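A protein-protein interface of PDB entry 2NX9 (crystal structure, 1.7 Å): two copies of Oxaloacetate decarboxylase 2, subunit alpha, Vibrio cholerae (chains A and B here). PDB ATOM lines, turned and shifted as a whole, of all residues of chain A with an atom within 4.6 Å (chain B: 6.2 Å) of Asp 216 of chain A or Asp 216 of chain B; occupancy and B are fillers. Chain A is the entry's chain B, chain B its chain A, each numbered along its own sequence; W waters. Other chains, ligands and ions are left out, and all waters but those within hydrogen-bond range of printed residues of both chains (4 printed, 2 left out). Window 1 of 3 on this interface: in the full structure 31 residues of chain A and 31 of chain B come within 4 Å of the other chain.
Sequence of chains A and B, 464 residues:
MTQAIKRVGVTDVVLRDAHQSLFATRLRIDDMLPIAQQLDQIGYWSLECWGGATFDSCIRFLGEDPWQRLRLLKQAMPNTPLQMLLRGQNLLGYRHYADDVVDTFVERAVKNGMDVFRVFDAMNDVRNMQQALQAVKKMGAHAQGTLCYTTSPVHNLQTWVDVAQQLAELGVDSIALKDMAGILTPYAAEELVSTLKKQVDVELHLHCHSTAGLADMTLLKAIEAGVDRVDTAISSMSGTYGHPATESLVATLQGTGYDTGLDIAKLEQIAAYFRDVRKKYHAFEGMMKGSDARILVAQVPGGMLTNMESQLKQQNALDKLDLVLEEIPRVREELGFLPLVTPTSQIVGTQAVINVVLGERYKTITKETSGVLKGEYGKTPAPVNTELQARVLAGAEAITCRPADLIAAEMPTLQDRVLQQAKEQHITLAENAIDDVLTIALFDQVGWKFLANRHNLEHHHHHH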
ATOM      1  N   GLY A 213      -0.856  17.383  13.515  1.00  0.00           N
ATOM      2  CA  GLY A 213      -0.940  17.531  14.963  1.00  0.00           C
ATOM      3  C   GLY A 213      -0.747  18.929  15.541  1.00  0.00           C
ATOM      4  O   GLY A 213      -0.564  19.073  16.748  1.00  0.00           O
ATOM      5  N   LEU A 214      -0.791  19.961  14.701  1.00  0.00           N
ATOM      6  CA  LEU A 214      -0.415  21.312  15.169  1.00  0.00           C
ATOM      7  C   LEU A 214      -1.615  22.218  15.408  1.00  0.00           C
ATOM      8  O   LEU A 214      -1.515  23.189  16.155  1.00  0.00           O
ATOM      9  CB  LEU A 214       0.567  22.006  14.203  1.00  0.00           C
ATOM     10  CG  LEU A 214       1.925  21.401  13.865  1.00  0.00           C
ATOM     11  CD1 LEU A 214       2.580  22.139  12.706  1.00  0.00           C
ATOM     12  CD2 LEU A 214       2.835  21.331  15.059  1.00  0.00           C
ATOM     13  N   ALA A 215      -2.738  21.890  14.792  1.00  0.00           N
ATOM     14  CA  ALA A 215      -3.849  22.830  14.667  1.00  0.00           C
ATOM     15  C   ALA A 215      -4.500  23.319  15.969  1.00  0.00           C
ATOM     16  O   ALA A 215      -4.875  24.498  16.060  1.00  0.00           O
ATOM     17  CB  ALA A 215      -4.890  22.284  13.726  1.00  0.00           C
ATOM     18  N   ASP A 216      -4.687  22.422  16.941  1.00  0.00           N
ATOM     19  CA  ASP A 216      -5.258  22.777  18.247  1.00  0.00           C
ATOM     20  C   ASP A 216      -4.425  23.865  18.925  1.00  0.00           C
ATOM     21  O   ASP A 216      -4.936  24.899  19.355  1.00  0.00           O
ATOM     22  CB  ASP A 216      -5.231  21.571  19.199  1.00  0.00           C
ATOM     23  CG  ASP A 216      -6.239  20.481  18.849  1.00  0.00           C
ATOM     24  OD1 ASP A 216      -6.935  20.519  17.800  1.00  0.00           O
ATOM     25  OD2 ASP A 216      -6.364  19.569  19.695  1.00  0.00           O
ATOM     26  N   MET A 217      -3.132  23.594  19.033  1.00  0.00           N
ATOM     27  CA  MET A 217      -2.171  24.523  19.637  1.00  0.00           C
ATOM     28  C   MET A 217      -2.068  25.829  18.820  1.00  0.00           C
ATOM     29  O   MET A 217      -2.070  26.935  19.387  1.00  0.00           O
ATOM     30  CB  MET A 217      -0.829  23.833  19.794  1.00  0.00           C
ATOM     31  CG  MET A 217      -0.788  22.597  20.717  1.00  0.00           C
ATOM     32  SD  MET A 217       0.910  22.003  20.915  1.00  0.00           S
ATOM     33  CE  MET A 217       1.144  20.917  19.527  1.00  0.00           C
ATOM     34  N   THR A 218      -2.042  25.690  17.491  1.00  0.00           N
ATOM     35  CA  THR A 218      -1.997  26.822  16.570  1.00  0.00           C
ATOM     36  C   THR A 218      -3.192  27.744  16.719  1.00  0.00           C
ATOM     37  O   THR A 218      -3.002  28.952  16.791  1.00  0.00           O
ATOM     38  CB  THR A 218      -1.812  26.368  15.095  1.00  0.00           C
ATOM     39  OG1 THR A 218      -0.461  25.946  14.922  1.00  0.00           O
ATOM     40  CG2 THR A 218      -2.165  27.512  14.070  1.00  0.00           C
ATOM     41  N   LEU A 219      -4.397  27.186  16.806  1.00  0.00           N
ATOM     42  CA  LEU A 219      -5.588  28.012  16.995  1.00  0.00           C
ATOM     43  C   LEU A 219      -5.546  28.808  18.304  1.00  0.00           C
ATOM     44  O   LEU A 219      -5.927  29.973  18.327  1.00  0.00           O
ATOM     45  CB  LEU A 219      -6.865  27.177  16.925  1.00  0.00           C
ATOM     46  CG  LEU A 219      -7.756  27.295  15.682  1.00  0.00           C
ATOM     47  CD1 LEU A 219      -6.974  27.106  14.404  1.00  0.00           C
ATOM     48  CD2 LEU A 219      -8.929  26.322  15.789  1.00  0.00           C
ATOM     49  N   LEU A 220      -5.036  28.187  19.368  1.00  0.00           N
ATOM     50  CA  LEU A 220      -4.944  28.825  20.688  1.00  0.00           C
ATOM     51  C   LEU A 220      -3.914  29.968  20.697  1.00  0.00           C
ATOM     52  O   LEU A 220      -4.197  31.074  21.173  1.00  0.00           O
ATOM     53  CB  LEU A 220      -4.610  27.790  21.785  1.00  0.00           C
ATOM     54  CG  LEU A 220      -4.843  28.346  23.201  1.00  0.00           C
ATOM     55  CD1 LEU A 220      -6.265  28.978  23.358  1.00  0.00           C
ATOM     56  CD2 LEU A 220      -4.547  27.312  24.294  1.00  0.00           C
ATOM     57  N   PRO A 244      -9.495  21.116  14.259  1.00  0.00           N
ATOM     58  CA  PRO A 244      -9.743  21.112  15.708  1.00  0.00           C
ATOM     59  C   PRO A 244     -11.260  21.063  16.005  1.00  0.00           C
ATOM     60  O   PRO A 244     -12.098  21.529  15.218  1.00  0.00           O
ATOM     61  CB  PRO A 244      -9.175  22.451  16.174  1.00  0.00           C
ATOM     62  CG  PRO A 244      -8.062  22.725  15.213  1.00  0.00           C
ATOM     63  CD  PRO A 244      -8.637  22.282  13.887  1.00  0.00           C
ATOM     64  N   CYS B 208      -1.654  14.206  30.396  1.00  0.00           N
ATOM     65  CA  CYS B 208      -3.018  14.548  29.977  1.00  0.00           C
ATOM     66  C   CYS B 208      -3.410  13.719  28.790  1.00  0.00           C
ATOM     67  O   CYS B 208      -2.643  13.405  27.869  1.00  0.00           O
ATOM     68  CB  CYS B 208      -3.079  16.052  29.678  1.00  0.00           C
ATOM     69  SG  CYS B 208      -4.721  16.742  29.368  1.00  0.00           S
ATOM     70  N   SER B 210      -6.131  12.955  25.494  1.00  0.00           N
ATOM     71  CA  SER B 210      -6.696  13.725  24.384  1.00  0.00           C
ATOM     72  C   SER B 210      -8.143  13.497  24.205  1.00  0.00           C
ATOM     73  O   SER B 210      -8.760  14.016  23.282  1.00  0.00           O
ATOM     74  CB  SER B 210      -6.008  13.295  23.108  1.00  0.00           C
ATOM     75  OG  SER B 210      -4.617  13.450  23.263  1.00  0.00           O
ATOM     76  N   GLY B 213     -10.270  16.428  23.834  1.00  0.00           N
ATOM     77  CA  GLY B 213      -9.652  17.339  22.882  1.00  0.00           C
ATOM     78  C   GLY B 213      -8.889  18.522  23.449  1.00  0.00           C
ATOM     79  O   GLY B 213      -8.754  19.547  22.754  1.00  0.00           O
ATOM     80  N   LEU B 214      -8.340  18.391  24.667  1.00  0.00           N
ATOM     81  CA  LEU B 214      -7.890  19.566  25.398  1.00  0.00           C
ATOM     82  C   LEU B 214      -6.431  19.455  25.551  1.00  0.00           C
ATOM     83  O   LEU B 214      -5.788  20.472  25.800  1.00  0.00           O
ATOM     84  CB  LEU B 214      -8.512  19.625  26.807  1.00  0.00           C
ATOM     85  CG  LEU B 214     -10.040  19.747  26.877  1.00  0.00           C
ATOM     86  CD1 LEU B 214     -10.481  19.805  28.303  1.00  0.00           C
ATOM     87  CD2 LEU B 214     -10.386  21.020  26.212  1.00  0.00           C
ATOM     88  N   ALA B 215      -5.934  18.214  25.395  1.00  0.00           N
ATOM     89  CA  ALA B 215      -4.609  17.845  25.781  1.00  0.00           C
ATOM     90  C   ALA B 215      -3.481  18.491  25.023  1.00  0.00           C
ATOM     91  O   ALA B 215      -2.456  18.742  25.601  1.00  0.00           O
ATOM     92  CB  ALA B 215      -4.424  16.293  25.750  1.00  0.00           C
ATOM     93  N   ASP B 216      -3.625  18.745  23.729  1.00  0.00           N
ATOM     94  CA  ASP B 216      -2.526  19.380  23.024  1.00  0.00           C
ATOM     95  C   ASP B 216      -2.367  20.821  23.554  1.00  0.00           C
ATOM     96  O   ASP B 216      -1.258  21.269  23.917  1.00  0.00           O
ATOM     97  CB  ASP B 216      -2.741  19.440  21.518  1.00  0.00           C
ATOM     98  CG  ASP B 216      -2.914  18.051  20.838  1.00  0.00           C
ATOM     99  OD1 ASP B 216      -2.817  16.989  21.484  1.00  0.00           O
ATOM    100  OD2 ASP B 216      -3.103  18.055  19.597  1.00  0.00           O
ATOM    101  N   MET B 217      -3.481  21.551  23.579  1.00  0.00           N
ATOM    102  CA  MET B 217      -3.483  22.929  24.096  1.00  0.00           C
ATOM    103  C   MET B 217      -3.036  23.026  25.539  1.00  0.00           C
ATOM    104  O   MET B 217      -2.297  23.926  25.950  1.00  0.00           O
ATOM    105  CB  MET B 217      -4.879  23.514  23.994  1.00  0.00           C
ATOM    106  CG  MET B 217      -5.329  23.795  22.539  1.00  0.00           C
ATOM    107  SD  MET B 217      -6.978  24.463  22.253  1.00  0.00           S
ATOM    108  CE  MET B 217      -7.974  23.094  22.791  1.00  0.00           C
ATOM    109  N   THR B 218      -3.531  22.088  26.415  1.00  0.00           N
ATOM    110  CA  THR B 218      -3.143  21.962  27.836  1.00  0.00           C
ATOM    111  C   THR B 218      -1.668  21.803  28.033  1.00  0.00           C
ATOM    112  O   THR B 218      -1.053  22.544  28.801  1.00  0.00           O
ATOM    113  CB  THR B 218      -3.950  20.853  28.517  1.00  0.00           C
ATOM    114  OG1 THR B 218      -5.307  21.228  28.584  1.00  0.00           O
ATOM    115  CG2 THR B 218      -3.453  20.522  29.921  1.00  0.00           C
ATOM    116  N   LEU B 219      -1.001  20.831  27.323  1.00  0.00           N
ATOM    117  CA  LEU B 219       0.457  20.638  27.506  1.00  0.00           C
ATOM    118  C   LEU B 219       1.204  21.910  27.130  1.00  0.00           C
ATOM    119  O   LEU B 219       2.223  22.208  27.737  1.00  0.00           O
ATOM    120  CB  LEU B 219       1.071  19.494  26.682  1.00  0.00           C
ATOM    121  CG  LEU B 219       0.937  18.050  27.191  1.00  0.00           C
ATOM    122  CD1 LEU B 219      -0.539  17.714  27.423  1.00  0.00           C
ATOM    123  CD2 LEU B 219       1.525  17.184  26.080  1.00  0.00           C
ATOM    124  N   LEU B 220       0.759  22.591  26.086  1.00  0.00           N
ATOM    125  CA  LEU B 220       1.400  23.836  25.632  1.00  0.00           C
ATOM    126  C   LEU B 220       1.235  24.974  26.644  1.00  0.00           C
ATOM    127  O   LEU B 220       2.204  25.633  26.960  1.00  0.00           O
ATOM    128  CB  LEU B 220       0.942  24.270  24.242  1.00  0.00           C
ATOM    129  CG  LEU B 220       1.520  25.567  23.654  1.00  0.00           C
ATOM    130  CD1 LEU B 220       2.987  25.400  23.385  1.00  0.00           C
ATOM    131  CD2 LEU B 220       0.840  25.884  22.368  1.00  0.00           C
ATOM    132  N   LYS B 221       0.037  25.180  27.171  1.00  0.00           N
ATOM    133  CA  LYS B 221      -0.123  26.147  28.269  1.00  0.00           C
ATOM    134  C   LYS B 221       0.632  25.801  29.581  1.00  0.00           C
ATOM    135  O   LYS B 221       1.091  26.716  30.271  1.00  0.00           O
ATOM    136  CB  LYS B 221      -1.604  26.481  28.521  1.00  0.00           C
ATOM    137  CG  LYS B 221      -2.440  27.167  27.386  1.00  0.00           C
ATOM    138  CD  LYS B 221      -1.832  28.473  26.811  1.00  0.00           C
ATOM    139  CE  LYS B 221      -1.518  29.494  27.892  1.00  0.00           C
ATOM    140  NZ  LYS B 221      -0.971  30.736  27.275  1.00  0.00           N
ATOM    141  N   HIS B 243      -3.005  10.342  23.712  1.00  0.00           N
ATOM    142  CA  HIS B 243      -2.194  11.474  24.204  1.00  0.00           C
ATOM    143  C   HIS B 243      -1.771  12.344  23.002  1.00  0.00           C
ATOM    144  O   HIS B 243      -1.929  11.897  21.849  1.00  0.00           O
ATOM    145  CB  HIS B 243      -0.890  10.929  24.844  1.00  0.00           C
ATOM    146  CG  HIS B 243      -1.118   9.842  25.840  1.00  0.00           C
ATOM    147  ND1 HIS B 243      -1.132   8.507  25.494  1.00  0.00           N
ATOM    148  CD2 HIS B 243      -1.424   9.893  27.154  1.00  0.00           C
ATOM    149  CE1 HIS B 243      -1.460   7.791  26.546  1.00  0.00           C
ATOM    150  NE2 HIS B 243      -1.635   8.610  27.564  1.00  0.00           N
ATOM    151  N   PRO B 244      -1.222  13.583  23.255  1.00  0.00           N
ATOM    152  CA  PRO B 244      -0.705  14.432  22.184  1.00  0.00           C
ATOM    153  C   PRO B 244       0.478  13.775  21.517  1.00  0.00           C
ATOM    154  O   PRO B 244       1.217  13.041  22.175  1.00  0.00           O
ATOM    155  CB  PRO B 244      -0.203  15.690  22.931  1.00  0.00           C
ATOM    156  CG  PRO B 244      -1.009  15.724  24.181  1.00  0.00           C
ATOM    157  CD  PRO B 244      -1.098  14.261  24.570  1.00  0.00           C
ATOM    158  N   ALA B 245       0.687  14.044  20.232  1.00  0.00           N
ATOM    159  CA  ALA B 245       1.848  13.473  19.530  1.00  0.00           C
ATOM    160  C   ALA B 245       3.141  14.108  19.954  1.00  0.00           C
ATOM    161  O   ALA B 245       3.240  15.324  20.106  1.00  0.00           O
ATOM    162  CB  ALA B 245       1.719  13.608  18.044  1.00  0.00           C
ATOM    163  N   SER B 248       4.678  16.541  17.140  1.00  0.00           N
ATOM    164  CA  SER B 248       3.893  17.760  17.064  1.00  0.00           C
ATOM    165  C   SER B 248       4.317  18.774  18.113  1.00  0.00           C
ATOM    166  O   SER B 248       4.474  19.960  17.795  1.00  0.00           O
ATOM    167  CB  SER B 248       2.415  17.437  17.228  1.00  0.00           C
ATOM    168  OG  SER B 248       1.977  16.624  16.156  1.00  0.00           O
ATOM    169  N   LEU B 249       4.519  18.306  19.347  1.00  0.00           N
ATOM    170  CA  LEU B 249       4.962  19.164  20.428  1.00  0.00           C
ATOM    171  C   LEU B 249       6.483  19.402  20.298  1.00  0.00           C
ATOM    172  O   LEU B 249       7.019  20.460  20.678  1.00  0.00           O
ATOM    173  CB  LEU B 249       4.549  18.587  21.792  1.00  0.00           C
ATOM    174  CG  LEU B 249       4.887  19.482  23.001  1.00  0.00           C
ATOM    175  CD1 LEU B 249       3.872  20.605  23.174  1.00  0.00           C
ATOM    176  CD2 LEU B 249       4.988  18.684  24.272  1.00  0.00           C
HETATM  177  O   HOH W   1      -8.087  24.284  19.123  1.00  0.00           O
HETATM  178  O   HOH W   2      -9.230  19.940  19.997  1.00  0.00           O
HETATM  179  O   HOH W   3       0.970  18.954  23.014  1.00  0.00           O
HETATM  180  O   HOH W   4      -0.483  17.146  18.641  1.00  0.00           O
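The backbone carbonyl oxygen (O) of Leu 214 of chain A sits at hydrogen-bond distance from the side-chain hydroxyl (OG1) of Thr 218 of chain A, 3.2 Å away.
O of Asp 216 of chain B sits close to SD of Met 217 of chain A. The backbone carbonyl oxygen (O) of Asp 216 of chain A lies close to the side-chain sulfur (SD) of Met 217 of chain B (3.6 Å).
Of chain B, only Gly 213 (3.9 Å), Asp 216 (3.6 Å) and Met 217 (3.4 Å) come within 4 Å of Asp 216 of chain A. Of chain A, only Gly 213 (3.9 Å), Asp 216 (3.6 Å) and Met 217 (3.5 Å) come within 4 Å of Asp 216 of chain B. Of the printed residues of chain B, Met 217 of chain A touches Asp 216 (3.5 Å), Leu 220 (3.7 Å), Ser 248 (3.9 Å) and Leu 249 (3.98 Å). Of the printed residues of chain A, Ser 248 of chain B touches Gly 213 (3.3 Å), Leu 214 (3.5 Å) and Met 217 (3.9 Å). Of the printed residues of chain A, Leu 249 of chain B touches Met 217. Thr 218 of chain B touches none of the printed residues of chain A. Pro 244 of chain B touches none of the printed residues of chain A. The nearest printed residue of chain A that does not touch Asp 216 of chain B is Leu 214 of chain A (5.7 Å).
Water W4 bridges O of Gly 213 of chain A (2.7 Å) and OD2 of Asp 216 of chain B (2.9 Å). Water W2 bridges the backbone carbonyl oxygen (O) of Gly 213 of chain B (2.8 Å) and the side-chain carboxylate (OD2) of Asp 216 of chain A (2.9 Å). Water W1 lies within hydrogen-bond range of the backbone carbonyl oxygen (O) of Asp 216 of chain A (3.2 Å) and the side-chain sulfur (SD) of Met 217 of chain B (3.3 Å). Water W3 bridges the backbone carbonyl oxygen (O) of Asp 216 of chain B (3.3 Å) and the side-chain sulfur (SD) of Met 217 of chain A (3.7 Å).
Gly 213 of chain A touches Asp 216 of chain B, and with the chains exchanged Asp 216 of chain A touches Gly 213 of chain B. Asp 216 of chain A touches its own counterpart, Asp 216 of chain B. Asp 216 of chain A touches Met 217 of chain B, and with the chains exchanged Met 217 of chain A touches Asp 216 of chain B. Met 217 of chain A touches Leu 220 of chain B, and with the chains exchanged Leu 220 of chain A touches Met 217 of chain B. 9 positions are printed for both chains.
Of the 9 printed residues of chain A, 5 touch a printed residue of chain B. Hydrophobic or aromatic side chains of chain A within 4 Å of the printed part of chain B: Leu 214, Met 217 and Leu 220. Printed residues of chain B that touch a printed residue of chain A: Gly 213, Asp 216, Met 217, Leu 220, Lys 221, Ser 248 and Leu 249. Hydrophobic or aromatic side chains of chain B within 4 Å of the printed part of chain A: Met 217, Leu 220 and Leu 249. Along chain B the printed residues that touch a printed residue of chain A span positions 213 to 249. Among the printed residues, no Asp or Glu carboxylate lies within 4 Å of a Lys or Arg side-chain nitrogen of the other chain.
O of Gly 213 of chain A touches OD2 of Asp 216 of chain B (3.9 Å). Ser 248 of chain B touches Gly 213 of chain A. Leu 214 of chain A touches Ser 248 of chain B. O of Gly 213 of chain B touches OD2 of Asp 216 of chain A, 3.9 Å away. Asp 216 of chain A touches Asp 216 of chain B (OD2 to OD2, 3.6 Å). Met 217 of chain A touches Leu 220 of chain B (CB to CD2, 3.7 Å). Ser 248 of chain B touches Met 217 of chain A. Leu 249 of chain B touches Met 217 of chain A. Leu 220 of chain A touches Met 217 of chain B. Lys 221 of chain B touches Leu 220 of chain A (CG to CD2, 3.7 Å).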
